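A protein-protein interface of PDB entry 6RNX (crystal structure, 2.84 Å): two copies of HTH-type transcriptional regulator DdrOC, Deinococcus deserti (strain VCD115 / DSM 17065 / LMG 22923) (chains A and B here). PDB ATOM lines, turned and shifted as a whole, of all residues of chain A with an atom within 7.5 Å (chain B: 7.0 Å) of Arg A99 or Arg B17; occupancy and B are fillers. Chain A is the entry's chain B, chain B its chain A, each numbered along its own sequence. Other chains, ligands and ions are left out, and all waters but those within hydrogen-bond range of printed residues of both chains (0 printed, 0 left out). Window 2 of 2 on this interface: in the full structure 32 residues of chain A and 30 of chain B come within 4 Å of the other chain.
The backbone carbonyl oxygen of Gly B15 lies within hydrogen-bond range of the guanidinium group of Arg A99 (2.6 Å).
OE2 of Glu B13 lies within salt-bridge range of NH1 of Arg B14, at 2.8 Å.
N of Arg B17 is in hydrogen-bond range of OD2 of Asp B20, at 2.9 Å.
The guanidinium group (NH1) of Arg A99 is in salt-bridge range of the side-chain carboxylate (OD2) of Asp A96.
The backbone carbonyl oxygen of Arg A99 sits at hydrogen-bond distance from the side-chain hydroxyl of Ser A102 (2.7 Å).
Among the printed residues, merely in contact across the chains: Pro A95 with Ser B12 (3.1 Å), Val A98 with Arg B14 (3.3 Å), Pro A95 with Gly B15 (3.5 Å), Pro A95 with Glu B13 (3.6 Å), Leu A76 with Arg B14 (3.7 Å), Arg A99 with Arg B17 (3.7 Å) and Val A98 with Glu B13 (3.8 Å).
Arg A99 touches two residues of chain B.
Of the printed residues of chain A, Ser B12 touches Pro A95 (3.1 Å).
Printed residues of chain A within 4 Å of Arg B14: Leu A76 (3.7 Å) and Val A98 (3.3 Å).
Printed residues of chain A within 4 Å of Gly B15: Pro A95 (3.5 Å) and Arg A99 (2.6 Å).
Of chain A, only Arg A99 (3.7 Å) comes within 4 Å of Arg B17.
Leu B18 touches none of the printed residues of chain A.
The nearest residue of chain B that does not touch Arg A99 is Leu B16 (4.1 Å).
The nearest residue of chain A that does not touch Arg B17 is Arg A103 (5.2 Å).
Of the 15 printed residues of chain B, 5 touch a printed residue of chain A.
Of the 14 printed residues of chain A, 4 touch a printed residue of chain B.
Printed residues of chain A that touch a printed residue of chain B: Leu A76, Pro A95, Val A98 and Arg A99.
Hydrophobic or aromatic side chains of chain A within 4 Å of the printed part of chain B: Leu A76, Pro A95 and Val A98.
No position is printed for both chains.
Of the 8 pairs that touch across the chains among the printed residues, none has its exchanged pair printed and touching as well.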
ATOM      1  N   LEU A  76      21.321 -13.821 -18.001  1.00  0.00           N
ATOM      2  CA  LEU A  76      20.234 -13.975 -17.057  1.00  0.00           C
ATOM      3  C   LEU A  76      20.185 -15.422 -16.592  1.00  0.00           C
ATOM      4  O   LEU A  76      20.826 -16.294 -17.183  1.00  0.00           O
ATOM      5  CB  LEU A  76      18.892 -13.596 -17.703  1.00  0.00           C
ATOM      6  CG  LEU A  76      18.519 -12.117 -17.763  1.00  0.00           C
ATOM      7  CD1 LEU A  76      17.044 -11.924 -18.076  1.00  0.00           C
ATOM      8  CD2 LEU A  76      18.890 -11.431 -16.457  1.00  0.00           C
ATOM      9  N   LEU A  80      14.380 -17.375 -15.537  1.00  0.00           N
ATOM     10  CA  LEU A  80      14.025 -15.967 -15.650  1.00  0.00           C
ATOM     11  C   LEU A  80      13.875 -15.571 -17.108  1.00  0.00           C
ATOM     12  O   LEU A  80      12.943 -14.845 -17.468  1.00  0.00           O
ATOM     13  CB  LEU A  80      15.079 -15.106 -14.962  1.00  0.00           C
ATOM     14  CG  LEU A  80      14.822 -13.621 -14.717  1.00  0.00           C
ATOM     15  CD1 LEU A  80      13.414 -13.356 -14.294  1.00  0.00           C
ATOM     16  CD2 LEU A  80      15.781 -13.121 -13.658  1.00  0.00           C
ATOM     17  N   ILE A  93       5.569  -8.360 -17.382  1.00  0.00           N
ATOM     18  CA  ILE A  93       6.707  -7.991 -16.552  1.00  0.00           C
ATOM     19  C   ILE A  93       7.558  -6.950 -17.260  1.00  0.00           C
ATOM     20  O   ILE A  93       7.892  -7.090 -18.446  1.00  0.00           O
ATOM     21  CB  ILE A  93       7.549  -9.223 -16.215  1.00  0.00           C
ATOM     22  CG1 ILE A  93       6.673 -10.294 -15.581  1.00  0.00           C
ATOM     23  CG2 ILE A  93       8.630  -8.832 -15.283  1.00  0.00           C
ATOM     24  CD1 ILE A  93       6.768 -11.633 -16.266  1.00  0.00           C
ATOM     25  N   THR A  94       7.944  -5.879 -16.492  1.00  0.00           N
ATOM     26  CA  THR A  94       8.780  -4.798 -16.984  1.00  0.00           C
ATOM     27  C   THR A  94      10.250  -5.185 -16.921  1.00  0.00           C
ATOM     28  O   THR A  94      10.662  -5.953 -16.043  1.00  0.00           O
ATOM     29  CB  THR A  94       8.603  -3.533 -16.149  1.00  0.00           C
ATOM     30  OG1 THR A  94       8.939  -3.796 -14.770  1.00  0.00           O
ATOM     31  CG2 THR A  94       7.190  -3.012 -16.273  1.00  0.00           C
ATOM     32  N   PRO A  95      11.039  -4.594 -17.824  1.00  0.00           N
ATOM     33  CA  PRO A  95      12.507  -4.706 -17.731  1.00  0.00           C
ATOM     34  C   PRO A  95      13.098  -4.577 -16.322  1.00  0.00           C
ATOM     35  O   PRO A  95      14.059  -5.276 -15.941  1.00  0.00           O
ATOM     36  CB  PRO A  95      12.953  -3.582 -18.664  1.00  0.00           C
ATOM     37  CG  PRO A  95      11.884  -3.541 -19.710  1.00  0.00           C
ATOM     38  CD  PRO A  95      10.601  -3.891 -19.042  1.00  0.00           C
ATOM     39  N   ASP A  96      12.480  -3.763 -15.501  1.00  0.00           N
ATOM     40  CA  ASP A  96      13.103  -3.415 -14.238  1.00  0.00           C
ATOM     41  C   ASP A  96      12.510  -4.199 -13.088  1.00  0.00           C
ATOM     42  O   ASP A  96      13.017  -4.195 -11.957  1.00  0.00           O
ATOM     43  CB  ASP A  96      12.935  -1.924 -14.135  1.00  0.00           C
ATOM     44  CG  ASP A  96      14.190  -1.218 -14.567  1.00  0.00           C
ATOM     45  OD1 ASP A  96      14.099  -0.318 -15.303  1.00  0.00           O
ATOM     46  OD2 ASP A  96      15.296  -1.535 -14.064  1.00  0.00           O
ATOM     47  N   TRP A  97      11.432  -4.908 -13.373  1.00  0.00           N
ATOM     48  CA  TRP A  97      11.157  -6.068 -12.554  1.00  0.00           C
ATOM     49  C   TRP A  97      12.130  -7.191 -12.891  1.00  0.00           C
ATOM     50  O   TRP A  97      12.546  -7.947 -12.001  1.00  0.00           O
ATOM     51  CB  TRP A  97       9.702  -6.480 -12.737  1.00  0.00           C
ATOM     52  CG  TRP A  97       8.902  -5.935 -11.604  1.00  0.00           C
ATOM     53  CD1 TRP A  97       8.085  -4.843 -11.612  1.00  0.00           C
ATOM     54  CD2 TRP A  97       8.929  -6.409 -10.262  1.00  0.00           C
ATOM     55  NE1 TRP A  97       7.578  -4.624 -10.357  1.00  0.00           N
ATOM     56  CE2 TRP A  97       8.076  -5.577  -9.509  1.00  0.00           C
ATOM     57  CE3 TRP A  97       9.590  -7.462  -9.626  1.00  0.00           C
ATOM     58  CZ2 TRP A  97       7.870  -5.763  -8.157  1.00  0.00           C
ATOM     59  CZ3 TRP A  97       9.384  -7.648  -8.307  1.00  0.00           C
ATOM     60  CH2 TRP A  97       8.531  -6.803  -7.572  1.00  0.00           C
ATOM     61  N   VAL A  98      12.553  -7.265 -14.157  1.00  0.00           N
ATOM     62  CA  VAL A  98      13.485  -8.309 -14.571  1.00  0.00           C
ATOM     63  C   VAL A  98      14.830  -8.141 -13.884  1.00  0.00           C
ATOM     64  O   VAL A  98      15.387  -9.108 -13.354  1.00  0.00           O
ATOM     65  CB  VAL A  98      13.640  -8.317 -16.093  1.00  0.00           C
ATOM     66  CG1 VAL A  98      14.645  -9.361 -16.485  1.00  0.00           C
ATOM     67  CG2 VAL A  98      12.294  -8.563 -16.739  1.00  0.00           C
ATOM     68  N   ARG A  99      15.384  -6.918 -13.908  1.00  0.00           N
ATOM     69  CA  ARG A  99      16.591  -6.612 -13.131  1.00  0.00           C
ATOM     70  C   ARG A  99      16.407  -6.963 -11.658  1.00  0.00           C
ATOM     71  O   ARG A  99      17.272  -7.598 -11.043  1.00  0.00           O
ATOM     72  CB  ARG A  99      16.957  -5.127 -13.242  1.00  0.00           C
ATOM     73  CG  ARG A  99      17.819  -4.710 -14.407  1.00  0.00           C
ATOM     74  CD  ARG A  99      18.163  -3.217 -14.327  1.00  0.00           C
ATOM     75  NE  ARG A  99      18.731  -2.689 -15.570  1.00  0.00           N
ATOM     76  CZ  ARG A  99      18.035  -2.028 -16.497  1.00  0.00           C
ATOM     77  NH1 ARG A  99      16.739  -1.821 -16.332  1.00  0.00           N
ATOM     78  NH2 ARG A  99      18.630  -1.583 -17.600  1.00  0.00           N
ATOM     79  N   THR A 100      15.283  -6.521 -11.077  1.00  0.00           N
ATOM     80  CA  THR A 100      15.015  -6.722  -9.656  1.00  0.00           C
ATOM     81  C   THR A 100      15.059  -8.184  -9.280  1.00  0.00           C
ATOM     82  O   THR A 100      15.579  -8.542  -8.216  1.00  0.00           O
ATOM     83  CB  THR A 100      13.655  -6.138  -9.309  1.00  0.00           C
ATOM     84  OG1 THR A 100      13.624  -4.765  -9.688  1.00  0.00           O
ATOM     85  CG2 THR A 100      13.374  -6.270  -7.846  1.00  0.00           C
ATOM     86  N   LEU A 101      14.514  -9.048 -10.135  1.00  0.00           N
ATOM     87  CA  LEU A 101      14.471 -10.467  -9.822  1.00  0.00           C
ATOM     88  C   LEU A 101      15.866 -11.094  -9.814  1.00  0.00           C
ATOM     89  O   LEU A 101      16.175 -11.911  -8.939  1.00  0.00           O
ATOM     90  CB  LEU A 101      13.557 -11.183 -10.816  1.00  0.00           C
ATOM     91  CG  LEU A 101      12.077 -10.796 -10.723  1.00  0.00           C
ATOM     92  CD1 LEU A 101      11.272 -11.592 -11.720  1.00  0.00           C
ATOM     93  CD2 LEU A 101      11.523 -10.981  -9.311  1.00  0.00           C
ATOM     94  N   SER A 102      16.732 -10.695 -10.759  1.00  0.00           N
ATOM     95  CA  SER A 102      17.979 -11.419 -11.020  1.00  0.00           C
ATOM     96  C   SER A 102      18.941 -11.383  -9.832  1.00  0.00           C
ATOM     97  O   SER A 102      19.763 -12.294  -9.669  1.00  0.00           O
ATOM     98  CB  SER A 102      18.643 -10.851 -12.275  1.00  0.00           C
ATOM     99  OG  SER A 102      18.813  -9.446 -12.171  1.00  0.00           O
ATOM    100  N   ARG A 103      18.848 -10.362  -8.994  1.00  0.00           N
ATOM    101  CA  ARG A 103      19.678 -10.280  -7.805  1.00  0.00           C
ATOM    102  C   ARG A 103      19.276 -11.264  -6.701  1.00  0.00           C
ATOM    103  O   ARG A 103      19.860 -11.208  -5.593  1.00  0.00           O
ATOM    104  CB  ARG A 103      19.655  -8.849  -7.273  1.00  0.00           C
ATOM    105  CG  ARG A 103      20.029  -7.837  -8.319  1.00  0.00           C
ATOM    106  CD  ARG A 103      20.533  -6.554  -7.699  1.00  0.00           C
ATOM    107  NE  ARG A 103      19.481  -5.555  -7.717  1.00  0.00           N
ATOM    108  CZ  ARG A 103      19.391  -4.579  -8.616  1.00  0.00           C
ATOM    109  NH1 ARG A 103      20.307  -4.448  -9.581  1.00  0.00           N
ATOM    110  NH2 ARG A 103      18.380  -3.727  -8.541  1.00  0.00           N
ATOM    111  N   ILE A 104      18.319 -12.159  -6.926  1.00  0.00           N
ATOM    112  CA  ILE A 104      17.919 -13.130  -5.917  1.00  0.00           C
ATOM    113  C   ILE A 104      18.673 -14.415  -6.192  1.00  0.00           C
ATOM    114  O   ILE A 104      18.376 -15.147  -7.145  1.00  0.00           O
ATOM    115  CB  ILE A 104      16.407 -13.371  -5.885  1.00  0.00           C
ATOM    116  CG1 ILE A 104      15.669 -12.088  -5.549  1.00  0.00           C
ATOM    117  CG2 ILE A 104      16.096 -14.372  -4.817  1.00  0.00           C
ATOM    118  CD1 ILE A 104      14.211 -12.117  -5.932  1.00  0.00           C
ATOM    119  N   ARG B  11      17.471  -7.227 -25.395  1.00  0.00           N
ATOM    120  CA  ARG B  11      18.196  -6.725 -24.237  1.00  0.00           C
ATOM    121  C   ARG B  11      17.349  -5.764 -23.397  1.00  0.00           C
ATOM    122  O   ARG B  11      17.355  -5.848 -22.162  1.00  0.00           O
ATOM    123  CB  ARG B  11      19.491  -6.049 -24.683  1.00  0.00           C
ATOM    124  CG  ARG B  11      20.374  -5.640 -23.501  1.00  0.00           C
ATOM    125  CD  ARG B  11      21.514  -4.707 -23.869  1.00  0.00           C
ATOM    126  NE  ARG B  11      21.145  -3.728 -24.887  1.00  0.00           N
ATOM    127  CZ  ARG B  11      20.789  -2.470 -24.645  1.00  0.00           C
ATOM    128  NH1 ARG B  11      20.751  -2.008 -23.401  1.00  0.00           N
ATOM    129  NH2 ARG B  11      20.474  -1.676 -25.659  1.00  0.00           N
ATOM    130  N   SER B  12      16.609  -4.852 -24.039  1.00  0.00           N
ATOM    131  CA  SER B  12      15.824  -3.879 -23.281  1.00  0.00           C
ATOM    132  C   SER B  12      14.699  -4.554 -22.493  1.00  0.00           C
ATOM    133  O   SER B  12      14.520  -4.284 -21.298  1.00  0.00           O
ATOM    134  CB  SER B  12      15.264  -2.798 -24.212  1.00  0.00           C
ATOM    135  OG  SER B  12      14.901  -1.628 -23.478  1.00  0.00           O
ATOM    136  N   GLU B  13      13.921  -5.430 -23.142  1.00  0.00           N
ATOM    137  CA  GLU B  13      12.858  -6.121 -22.422  1.00  0.00           C
ATOM    138  C   GLU B  13      13.416  -6.935 -21.266  1.00  0.00           C
ATOM    139  O   GLU B  13      12.693  -7.212 -20.304  1.00  0.00           O
ATOM    140  CB  GLU B  13      12.044  -7.012 -23.376  1.00  0.00           C
ATOM    141  CG  GLU B  13      12.554  -8.451 -23.585  1.00  0.00           C
ATOM    142  CD  GLU B  13      11.875  -9.176 -24.766  1.00  0.00           C
ATOM    143  OE1 GLU B  13      11.105  -8.532 -25.514  1.00  0.00           O
ATOM    144  OE2 GLU B  13      12.119 -10.389 -24.961  1.00  0.00           O
ATOM    145  N   ARG B  14      14.696  -7.275 -21.319  1.00  0.00           N
ATOM    146  CA  ARG B  14      15.365  -8.053 -20.291  1.00  0.00           C
ATOM    147  C   ARG B  14      16.099  -7.197 -19.275  1.00  0.00           C
ATOM    148  O   ARG B  14      16.810  -7.749 -18.430  1.00  0.00           O
ATOM    149  CB  ARG B  14      16.369  -9.010 -20.928  1.00  0.00           C
ATOM    150  CG  ARG B  14      15.836 -10.379 -21.194  1.00  0.00           C
ATOM    151  CD  ARG B  14      16.746 -11.115 -22.142  1.00  0.00           C
ATOM    152  NE  ARG B  14      16.067 -12.235 -22.789  1.00  0.00           N
ATOM    153  CZ  ARG B  14      15.106 -12.096 -23.699  1.00  0.00           C
ATOM    154  NH1 ARG B  14      14.698 -10.881 -24.073  1.00  0.00           N
ATOM    155  NH2 ARG B  14      14.549 -13.176 -24.239  1.00  0.00           N
ATOM    156  N   GLY B  15      15.986  -5.874 -19.361  1.00  0.00           N
ATOM    157  CA  GLY B  15      16.587  -4.993 -18.371  1.00  0.00           C
ATOM    158  C   GLY B  15      18.102  -4.990 -18.326  1.00  0.00           C
ATOM    159  O   GLY B  15      18.687  -4.712 -17.276  1.00  0.00           O
ATOM    160  N   LEU B  16      18.765  -5.280 -19.438  1.00  0.00           N
ATOM    161  CA  LEU B  16      20.211  -5.414 -19.440  1.00  0.00           C
ATOM    162  C   LEU B  16      20.842  -4.188 -20.084  1.00  0.00           C
ATOM    163  O   LEU B  16      20.329  -3.669 -21.079  1.00  0.00           O
ATOM    164  CB  LEU B  16      20.623  -6.692 -20.170  1.00  0.00           C
ATOM    165  CG  LEU B  16      20.411  -8.014 -19.409  1.00  0.00           C
ATOM    166  CD1 LEU B  16      20.230  -9.185 -20.360  1.00  0.00           C
ATOM    167  CD2 LEU B  16      21.578  -8.303 -18.487  1.00  0.00           C
ATOM    168  N   ARG B  17      21.930  -3.704 -19.486  1.00  0.00           N
ATOM    169  CA  ARG B  17      22.721  -2.634 -20.076  1.00  0.00           C
ATOM    170  C   ARG B  17      23.649  -3.209 -21.147  1.00  0.00           C
ATOM    171  O   ARG B  17      24.003  -4.391 -21.120  1.00  0.00           O
ATOM    172  CB  ARG B  17      23.523  -1.901 -18.993  1.00  0.00           C
ATOM    173  CG  ARG B  17      22.775  -1.681 -17.675  1.00  0.00           C
ATOM    174  CD  ARG B  17      23.655  -0.957 -16.632  1.00  0.00           C
ATOM    175  NE  ARG B  17      23.390  -1.326 -15.232  1.00  0.00           N
ATOM    176  CZ  ARG B  17      22.333  -0.938 -14.517  1.00  0.00           C
ATOM    177  NH1 ARG B  17      21.406  -0.157 -15.049  1.00  0.00           N
ATOM    178  NH2 ARG B  17      22.199  -1.336 -13.259  1.00  0.00           N
ATOM    179  N   LEU B  18      24.036  -2.373 -22.114  1.00  0.00           N
ATOM    180  CA  LEU B  18      24.966  -2.864 -23.131  1.00  0.00           C
ATOM    181  C   LEU B  18      26.160  -3.580 -22.501  1.00  0.00           C
ATOM    182  O   LEU B  18      26.591  -4.623 -22.998  1.00  0.00           O
ATOM    183  CB  LEU B  18      25.447  -1.728 -24.043  1.00  0.00           C
ATOM    184  CG  LEU B  18      24.501  -1.255 -25.162  1.00  0.00           C
ATOM    185  CD1 LEU B  18      24.973   0.081 -25.697  1.00  0.00           C
ATOM    186  CD2 LEU B  18      24.313  -2.250 -26.307  1.00  0.00           C
ATOM    187  N   LYS B  19      26.682  -3.055 -21.386  1.00  0.00           N
ATOM    188  CA  LYS B  19      27.869  -3.659 -20.778  1.00  0.00           C
ATOM    189  C   LYS B  19      27.596  -5.088 -20.325  1.00  0.00           C
ATOM    190  O   LYS B  19      28.439  -5.972 -20.514  1.00  0.00           O
ATOM    191  CB  LYS B  19      28.376  -2.817 -19.600  1.00  0.00           C
ATOM    192  CG  LYS B  19      27.388  -2.704 -18.465  1.00  0.00           C
ATOM    193  CD  LYS B  19      28.050  -2.489 -17.122  1.00  0.00           C
ATOM    194  CE  LYS B  19      27.013  -2.009 -16.109  1.00  0.00           C
ATOM    195  NZ  LYS B  19      27.081  -0.536 -15.914  1.00  0.00           N
ATOM    196  N   ASP B  20      26.427  -5.337 -19.734  1.00  0.00           N
ATOM    197  CA  ASP B  20      26.132  -6.677 -19.251  1.00  0.00           C
ATOM    198  C   ASP B  20      26.276  -7.675 -20.386  1.00  0.00           C
ATOM    199  O   ASP B  20      26.964  -8.695 -20.259  1.00  0.00           O
ATOM    200  CB  ASP B  20      24.720  -6.737 -18.643  1.00  0.00           C
ATOM    201  CG  ASP B  20      24.493  -5.717 -17.532  1.00  0.00           C
ATOM    202  OD1 ASP B  20      25.437  -5.482 -16.763  1.00  0.00           O
ATOM    203  OD2 ASP B  20      23.368  -5.167 -17.412  1.00  0.00           O
ATOM    204  N   VAL B  21      25.643  -7.376 -21.514  1.00  0.00           N
ATOM    205  CA  VAL B  21      25.753  -8.235 -22.689  1.00  0.00           C
ATOM    206  C   VAL B  21      27.200  -8.298 -23.154  1.00  0.00           C
ATOM    207  O   VAL B  21      27.735  -9.374 -23.445  1.00  0.00           O
ATOM    208  CB  VAL B  21      24.825  -7.728 -23.810  1.00  0.00           C
ATOM    209  CG1 VAL B  21      24.953  -8.609 -25.023  1.00  0.00           C
ATOM    210  CG2 VAL B  21      23.374  -7.631 -23.330  1.00  0.00           C
ATOM    211  N   ALA B  22      27.854  -7.138 -23.221  1.00  0.00           N
ATOM    212  CA  ALA B  22      29.240  -7.070 -23.662  1.00  0.00           C
ATOM    213  C   ALA B  22      30.100  -8.103 -22.951  1.00  0.00           C
ATOM    214  O   ALA B  22      30.829  -8.861 -23.592  1.00  0.00           O
ATOM    215  CB  ALA B  22      29.799  -5.667 -23.424  1.00  0.00           C
ATOM    216  N   VAL B  29      31.220  -2.923 -26.280  1.00  0.00           N
ATOM    217  CA  VAL B  29      30.038  -2.067 -26.258  1.00  0.00           C
ATOM    218  C   VAL B  29      29.869  -1.310 -27.579  1.00  0.00           C
ATOM    219  O   VAL B  29      28.746  -1.286 -28.116  1.00  0.00           O
ATOM    220  CB  VAL B  29      30.095  -1.103 -25.062  1.00  0.00           C
ATOM    221  CG1 VAL B  29      29.193   0.096 -25.294  1.00  0.00           C
ATOM    222  CG2 VAL B  29      29.726  -1.832 -23.787  1.00  0.00           C
ATOM    223  N   LEU B  32      28.758  -4.013 -30.273  1.00  0.00           N
ATOM    224  CA  LEU B  32      27.390  -4.431 -29.996  1.00  0.00           C
ATOM    225  C   LEU B  32      26.423  -3.287 -30.277  1.00  0.00           C
ATOM    226  O   LEU B  32      25.394  -3.478 -30.939  1.00  0.00           O
ATOM    227  CB  LEU B  32      27.234  -4.942 -28.561  1.00  0.00           C
ATOM    228  CG  LEU B  32      25.752  -5.295 -28.269  1.00  0.00           C
ATOM    229  CD1 LEU B  32      25.205  -6.443 -29.141  1.00  0.00           C
ATOM    230  CD2 LEU B  32      25.521  -5.618 -26.822  1.00  0.00           C
ATOM    231  N   GLU B  36      23.146  -3.201 -32.684  1.00  0.00           N
ATOM    232  CA  GLU B  36      21.805  -2.790 -32.282  1.00  0.00           C
ATOM    233  C   GLU B  36      21.335  -1.544 -33.038  1.00  0.00           C
ATOM    234  O   GLU B  36      20.125  -1.279 -33.117  1.00  0.00           O
ATOM    235  CB  GLU B  36      21.767  -2.555 -30.766  1.00  0.00           C
ATOM    236  CG  GLU B  36      21.930  -3.792 -29.901  1.00  0.00           C
ATOM    237  CD  GLU B  36      21.577  -3.548 -28.434  1.00  0.00           C
ATOM    238  OE1 GLU B  36      21.326  -2.380 -28.068  1.00  0.00           O
ATOM    239  OE2 GLU B  36      21.557  -4.525 -27.653  1.00  0.00           O
